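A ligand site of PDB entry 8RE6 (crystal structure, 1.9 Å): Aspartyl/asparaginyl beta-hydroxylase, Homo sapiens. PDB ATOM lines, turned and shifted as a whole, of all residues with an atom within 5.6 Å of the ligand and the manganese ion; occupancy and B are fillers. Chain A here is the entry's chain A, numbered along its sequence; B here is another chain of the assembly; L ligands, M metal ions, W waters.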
ATOM      1  N   LEU A 305       4.214   4.789  10.026  1.00  0.00           N
ATOM      2  CA  LEU A 305       4.383   5.566  11.241  1.00  0.00           C
ATOM      3  C   LEU A 305       4.516   7.062  10.985  1.00  0.00           C
ATOM      4  O   LEU A 305       4.471   7.849  11.940  1.00  0.00           O
ATOM      5  CB  LEU A 305       5.608   5.073  12.017  1.00  0.00           C
ATOM      6  CG  LEU A 305       5.542   3.625  12.492  1.00  0.00           C
ATOM      7  CD1 LEU A 305       6.823   3.219  13.201  1.00  0.00           C
ATOM      8  CD2 LEU A 305       4.341   3.412  13.405  1.00  0.00           C
ATOM      9  N   TRP A 311      10.772  11.152   5.805  1.00  0.00           N
ATOM     10  CA  TRP A 311      11.490  10.420   6.832  1.00  0.00           C
ATOM     11  C   TRP A 311      12.068   9.163   6.201  1.00  0.00           C
ATOM     12  O   TRP A 311      11.314   8.338   5.680  1.00  0.00           O
ATOM     13  CB  TRP A 311      10.541  10.072   7.985  1.00  0.00           C
ATOM     14  CG  TRP A 311      11.045   9.140   9.045  1.00  0.00           C
ATOM     15  CD1 TRP A 311      12.347   8.920   9.411  1.00  0.00           C
ATOM     16  CD2 TRP A 311      10.241   8.322   9.900  1.00  0.00           C
ATOM     17  NE1 TRP A 311      12.397   7.998  10.429  1.00  0.00           N
ATOM     18  CE2 TRP A 311      11.120   7.609  10.750  1.00  0.00           C
ATOM     19  CE3 TRP A 311       8.865   8.106  10.019  1.00  0.00           C
ATOM     20  CZ2 TRP A 311      10.669   6.708  11.707  1.00  0.00           C
ATOM     21  CZ3 TRP A 311       8.415   7.205  10.976  1.00  0.00           C
ATOM     22  CH2 TRP A 311       9.308   6.525  11.807  1.00  0.00           C
ATOM     23  N   GLN A 313      15.609   6.170   6.162  1.00  0.00           N
ATOM     24  CA  GLN A 313      16.617   5.507   6.971  1.00  0.00           C
ATOM     25  C   GLN A 313      17.565   4.720   6.080  1.00  0.00           C
ATOM     26  O   GLN A 313      17.171   4.175   5.046  1.00  0.00           O
ATOM     27  CB  GLN A 313      15.986   4.553   7.999  1.00  0.00           C
ATOM     28  CG  GLN A 313      15.120   5.224   9.053  1.00  0.00           C
ATOM     29  CD  GLN A 313      14.104   4.265   9.632  1.00  0.00           C
ATOM     30  OE1 GLN A 313      13.683   3.328   8.962  1.00  0.00           O
ATOM     31  NE2 GLN A 313      13.700   4.506  10.870  1.00  0.00           N
ATOM     32  N   LYS A 352      21.339   2.188  12.110  1.00  0.00           N
ATOM     33  CA  LYS A 352      20.878   2.875  10.908  1.00  0.00           C
ATOM     34  C   LYS A 352      20.966   4.378  11.077  1.00  0.00           C
ATOM     35  O   LYS A 352      20.816   4.903  12.184  1.00  0.00           O
ATOM     36  CB  LYS A 352      19.443   2.475  10.561  1.00  0.00           C
ATOM     37  CG  LYS A 352      18.439   2.718  11.687  1.00  0.00           C
ATOM     38  CD  LYS A 352      17.074   2.127  11.335  1.00  0.00           C
ATOM     39  CE  LYS A 352      16.110   2.211  12.511  1.00  0.00           C
ATOM     40  NZ  LYS A 352      14.814   1.525  12.229  1.00  0.00           N
ATOM     41  N   SER A 354      19.178   8.019  10.179  1.00  0.00           N
ATOM     42  CA  SER A 354      17.800   8.472  10.057  1.00  0.00           C
ATOM     43  C   SER A 354      17.790   9.947   9.673  1.00  0.00           C
ATOM     44  O   SER A 354      18.413  10.762  10.352  1.00  0.00           O
ATOM     45  CB  SER A 354      17.031   8.251  11.371  1.00  0.00           C
ATOM     46  OG  SER A 354      15.688   8.688  11.266  1.00  0.00           O
ATOM     47  N   MET A 356      15.227  13.219   8.807  1.00  0.00           N
ATOM     48  CA  MET A 356      13.907  13.829   8.813  1.00  0.00           C
ATOM     49  C   MET A 356      14.013  15.269   8.352  1.00  0.00           C
ATOM     50  O   MET A 356      14.900  16.011   8.802  1.00  0.00           O
ATOM     51  CB  MET A 356      13.291  13.782  10.209  1.00  0.00           C
ATOM     52  CG  MET A 356      12.875  12.405  10.621  1.00  0.00           C
ATOM     53  SD  MET A 356      12.086  12.426  12.230  1.00  0.00           S
ATOM     54  CE  MET A 356      11.712  10.700  12.374  1.00  0.00           C
ATOM     55  N   VAL A 362       6.051  12.201  13.284  1.00  0.00           N
ATOM     56  CA  VAL A 362       5.928  10.762  13.418  1.00  0.00           C
ATOM     57  C   VAL A 362       4.828  10.480  14.425  1.00  0.00           C
ATOM     58  O   VAL A 362       4.877  10.983  15.557  1.00  0.00           O
ATOM     59  CB  VAL A 362       7.256  10.123  13.839  1.00  0.00           C
ATOM     60  CG1 VAL A 362       7.087   8.630  14.074  1.00  0.00           C
ATOM     61  CG2 VAL A 362       8.301  10.372  12.788  1.00  0.00           C
ATOM     62  N   HIS A 365       3.965   6.083  18.713  1.00  0.00           N
ATOM     63  CA  HIS A 365       4.038   4.664  18.397  1.00  0.00           C
ATOM     64  C   HIS A 365       4.978   3.979  19.381  1.00  0.00           C
ATOM     65  O   HIS A 365       5.654   4.620  20.185  1.00  0.00           O
ATOM     66  CB  HIS A 365       4.496   4.430  16.961  1.00  0.00           C
ATOM     67  CG  HIS A 365       5.927   4.800  16.722  1.00  0.00           C
ATOM     68  ND1 HIS A 365       6.345   6.109  16.544  1.00  0.00           N
ATOM     69  CD2 HIS A 365       7.044   4.046  16.626  1.00  0.00           C
ATOM     70  CE1 HIS A 365       7.647   6.139  16.353  1.00  0.00           C
ATOM     71  NE2 HIS A 365       8.099   4.898  16.401  1.00  0.00           N
ATOM     72  N   ARG A 374      17.306   2.000  22.724  1.00  0.00           N
ATOM     73  CA  ARG A 374      17.584   2.706  21.485  1.00  0.00           C
ATOM     74  C   ARG A 374      18.428   3.940  21.785  1.00  0.00           C
ATOM     75  O   ARG A 374      17.995   4.830  22.509  1.00  0.00           O
ATOM     76  CB  ARG A 374      16.295   3.091  20.775  1.00  0.00           C
ATOM     77  CG  ARG A 374      16.503   3.742  19.418  1.00  0.00           C
ATOM     78  CD  ARG A 374      15.342   3.468  18.482  1.00  0.00           C
ATOM     79  NE  ARG A 374      15.459   2.185  17.804  1.00  0.00           N
ATOM     80  CZ  ARG A 374      14.690   1.811  16.782  1.00  0.00           C
ATOM     81  NH1 ARG A 374      13.726   2.593  16.317  1.00  0.00           N
ATOM     82  NH2 ARG A 374      14.922   0.635  16.206  1.00  0.00           N
ATOM     83  N   HIS A 376      20.345   7.319  20.253  1.00  0.00           N
ATOM     84  CA  HIS A 376      20.415   8.284  19.169  1.00  0.00           C
ATOM     85  C   HIS A 376      21.693   9.097  19.327  1.00  0.00           C
ATOM     86  O   HIS A 376      21.905   9.714  20.387  1.00  0.00           O
ATOM     87  CB  HIS A 376      19.214   9.228  19.152  1.00  0.00           C
ATOM     88  CG  HIS A 376      17.955   8.617  18.625  1.00  0.00           C
ATOM     89  ND1 HIS A 376      16.777   9.316  18.525  1.00  0.00           N
ATOM     90  CD2 HIS A 376      17.692   7.370  18.173  1.00  0.00           C
ATOM     91  CE1 HIS A 376      15.833   8.528  18.026  1.00  0.00           C
ATOM     92  NE2 HIS A 376      16.358   7.342  17.807  1.00  0.00           N
ATOM     93  N   ILE A 388      11.912  15.083  20.527  1.00  0.00           N
ATOM     94  CA  ILE A 388      11.421  13.720  20.641  1.00  0.00           C
ATOM     95  C   ILE A 388      10.796  13.554  22.015  1.00  0.00           C
ATOM     96  O   ILE A 388      11.401  13.910  23.034  1.00  0.00           O
ATOM     97  CB  ILE A 388      12.546  12.680  20.430  1.00  0.00           C
ATOM     98  CG1 ILE A 388      12.053  11.269  20.759  1.00  0.00           C
ATOM     99  CG2 ILE A 388      13.786  13.031  21.251  1.00  0.00           C
ATOM    100  CD1 ILE A 388      13.048  10.181  20.408  1.00  0.00           C
ATOM    101  N   PHE A 405      16.712   6.037  24.960  1.00  0.00           N
ATOM    102  CA  PHE A 405      15.360   5.814  25.429  1.00  0.00           C
ATOM    103  C   PHE A 405      14.952   4.375  25.108  1.00  0.00           C
ATOM    104  O   PHE A 405      15.576   3.700  24.288  1.00  0.00           O
ATOM    105  CB  PHE A 405      14.359   6.809  24.802  1.00  0.00           C
ATOM    106  CG  PHE A 405      14.230   6.694  23.307  1.00  0.00           C
ATOM    107  CD1 PHE A 405      15.191   7.231  22.467  1.00  0.00           C
ATOM    108  CD2 PHE A 405      13.132   6.064  22.754  1.00  0.00           C
ATOM    109  CE1 PHE A 405      15.065   7.126  21.088  1.00  0.00           C
ATOM    110  CE2 PHE A 405      12.996   5.957  21.386  1.00  0.00           C
ATOM    111  CZ  PHE A 405      13.965   6.492  20.552  1.00  0.00           C
ATOM    112  N   ASP A 407      12.339   2.413  23.344  1.00  0.00           N
ATOM    113  CA  ASP A 407      11.318   2.678  22.331  1.00  0.00           C
ATOM    114  C   ASP A 407      10.137   1.710  22.416  1.00  0.00           C
ATOM    115  O   ASP A 407       9.223   1.804  21.595  1.00  0.00           O
ATOM    116  CB  ASP A 407      11.929   2.685  20.923  1.00  0.00           C
ATOM    117  CG  ASP A 407      12.006   1.306  20.287  1.00  0.00           C
ATOM    118  OD1 ASP A 407      12.307   0.317  20.980  1.00  0.00           O
ATOM    119  OD2 ASP A 407      11.789   1.236  19.055  1.00  0.00           O
ATOM    120  N   HIS A 411       6.471   6.777  21.907  1.00  0.00           N
ATOM    121  CA  HIS A 411       7.320   7.922  21.617  1.00  0.00           C
ATOM    122  C   HIS A 411       6.869   8.576  20.323  1.00  0.00           C
ATOM    123  O   HIS A 411       6.111   8.014  19.538  1.00  0.00           O
ATOM    124  CB  HIS A 411       8.807   7.515  21.540  1.00  0.00           C
ATOM    125  CG  HIS A 411       9.096   6.415  20.575  1.00  0.00           C
ATOM    126  ND1 HIS A 411       8.789   5.102  20.829  1.00  0.00           N
ATOM    127  CD2 HIS A 411       9.686   6.438  19.350  1.00  0.00           C
ATOM    128  CE1 HIS A 411       9.157   4.359  19.802  1.00  0.00           C
ATOM    129  NE2 HIS A 411       9.708   5.137  18.899  1.00  0.00           N
ATOM    130  N   VAL A 413       7.961  12.091  17.460  1.00  0.00           N
ATOM    131  CA  VAL A 413       8.990  12.997  16.958  1.00  0.00           C
ATOM    132  C   VAL A 413       8.358  14.096  16.114  1.00  0.00           C
ATOM    133  O   VAL A 413       7.419  13.834  15.353  1.00  0.00           O
ATOM    134  CB  VAL A 413      10.061  12.235  16.139  1.00  0.00           C
ATOM    135  CG1 VAL A 413      11.043  13.192  15.502  1.00  0.00           C
ATOM    136  CG2 VAL A 413      10.811  11.242  17.031  1.00  0.00           C
ATOM    137  N   ILE A 423      20.396  11.770  12.331  1.00  0.00           N
ATOM    138  CA  ILE A 423      20.804  11.103  13.557  1.00  0.00           C
ATOM    139  C   ILE A 423      21.289   9.698  13.212  1.00  0.00           C
ATOM    140  O   ILE A 423      20.998   9.168  12.139  1.00  0.00           O
ATOM    141  CB  ILE A 423      19.670  11.033  14.613  1.00  0.00           C
ATOM    142  CG1 ILE A 423      18.490  10.227  14.087  1.00  0.00           C
ATOM    143  CG2 ILE A 423      19.242  12.432  15.034  1.00  0.00           C
ATOM    144  CD1 ILE A 423      17.457   9.909  15.144  1.00  0.00           C
ATOM    145  N   ILE A 425      21.169   5.858  14.736  1.00  0.00           N
ATOM    146  CA  ILE A 425      20.393   5.034  15.653  1.00  0.00           C
ATOM    147  C   ILE A 425      21.151   3.736  15.907  1.00  0.00           C
ATOM    148  O   ILE A 425      21.519   3.029  14.962  1.00  0.00           O
ATOM    149  CB  ILE A 425      18.988   4.742  15.098  1.00  0.00           C
ATOM    150  CG1 ILE A 425      18.282   6.044  14.730  1.00  0.00           C
ATOM    151  CG2 ILE A 425      18.181   3.958  16.119  1.00  0.00           C
ATOM    152  CD1 ILE A 425      16.869   5.861  14.265  1.00  0.00           C
ATOM    153  N   ASP B  18      10.680  -0.729  13.354  1.00  0.00           N
ATOM    154  CA  ASP B  18      10.307   0.381  14.211  1.00  0.00           C
ATOM    155  C   ASP B  18       8.991   0.181  14.943  1.00  0.00           C
ATOM    156  O   ASP B  18       8.779   0.822  15.980  1.00  0.00           O
ATOM    157  CB  ASP B  18      10.230   1.682  13.405  1.00  0.00           C
ATOM    158  CG  ASP B  18      11.589   2.125  12.890  1.00  0.00           C
ATOM    159  OD1 ASP B  18      12.580   1.943  13.628  1.00  0.00           O
ATOM    160  OD2 ASP B  18      11.652   2.653  11.761  1.00  0.00           O
HETATM  161  C1  LIG L   1      13.010   5.888  16.865  1.00  0.00           C
HETATM  162  O1  LIG L   1      14.224   6.056  16.976  1.00  0.00           O
HETATM  163  O2  LIG L   1      12.358   4.827  17.276  1.00  0.00           O
HETATM  164  C2  LIG L   1      12.144   6.954  16.199  1.00  0.00           C
HETATM  165  O3  LIG L   1      10.929   6.813  16.150  1.00  0.00           O
HETATM  166  C3  LIG L   1      12.862   8.113  15.581  1.00  0.00           C
HETATM  167  C4  LIG L   1      12.844   8.080  14.065  1.00  0.00           C
HETATM  168  C5  LIG L   1      13.486   6.872  13.441  1.00  0.00           C
HETATM  169  O4  LIG L   1      14.383   6.954  12.636  1.00  0.00           O
HETATM  170  O5  LIG L   1      12.974   5.729  13.825  1.00  0.00           O
HETATM  171 MN    MN M   1      10.306   4.780  16.889  1.00  0.00          MN
HETATM  172  O   HOH W   1      10.350   2.791  17.326  1.00  0.00           O
HETATM  173  O   HOH W   2      10.716   4.504  14.799  1.00  0.00           O
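The guanidinium group of Arg 374 lies within salt-bridge range of an oxygen (O1) of the ligand, 3.6 Å away. O4 of the ligand is in hydrogen-bond range of NE2 of Gln 313 (3.1 Å). The side-chain hydroxyl (OG) of Ser 354 sits at hydrogen-bond distance from an oxygen (O4) of the ligand (2.6 Å). O4 of the ligand is in hydrogen-bond range of NE1 of Trp 311, 3.1 Å away. A ring nitrogen (NE2) of His 376 lies within hydrogen-bond range of an oxygen (O1) of the ligand (2.6 Å).
OG of Ser 354 lies within hydrogen-bond range of NE1 of Trp 311 (3.5 Å). The side-chain carboxylate (OD1) of Asp 18 of chain B lies within salt-bridge range of the side-chain amino group (NZ) of Lys 352. The guanidinium group (NH1) of Arg 374 is in salt-bridge range of the side-chain carboxylate (OD1) of Asp 18 of chain B, at 3.0 Å. The backbone NH of Ser 354 lies within hydrogen-bond range of the backbone carbonyl oxygen of Ile 423. N of Ile 425 sits at hydrogen-bond distance from O of Lys 352 (2.7 Å). NE2 of Gln 313 sits close to NZ of Lys 352. A ring nitrogen (ND1) of His 411 lies close to the backbone carbonyl oxygen (O) of Asp 407. NH1 of Arg 374 lies within salt-bridge range of OD2 of Asp 407, at 3.6 Å.
Met 356 touches the ligand. CZ of Phe 405 touches O1 of the ligand (3.6 Å). Ile 425 touches the ligand. OD1 of Asp 18 of chain B touches O5 of the ligand, at 3.8 Å. Hydrophobic or aromatic side chains within 4 Å of the ligand: Trp 311, Met 356, His 365, His 376, Phe 405, His 411 and Ile 425. Within 4 Å of the ligand: Trp 311, Gln 313, Ser 354, Met 356, His 365, Arg 374, His 376, Phe 405, His 411, Ile 425 and Asp 18 of chain B.
Two residues have an atom within 4 Å of the manganese ion: His 365 and His 411. The nearest printed residue that does not touch the manganese ion is Arg 374 (4.1 Å).
The manganese ion is bound by water W1 (2.0 Å), O2 of the ligand (2.1 Å), NE2 of His 411 (2.1 Å), water W2 (2.1 Å), O3 of the ligand (2.3 Å) and NE2 of His 365 (2.3 Å).
Water W1 bridges the side-chain carboxylate of Asp 407 (2.7 Å) and the backbone carbonyl oxygen of Asp 18 of chain B (2.9 Å). Water W2 bridges O5 of the ligand (2.7 Å) and OD1 of Asp 18 of chain B (3.4 Å).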
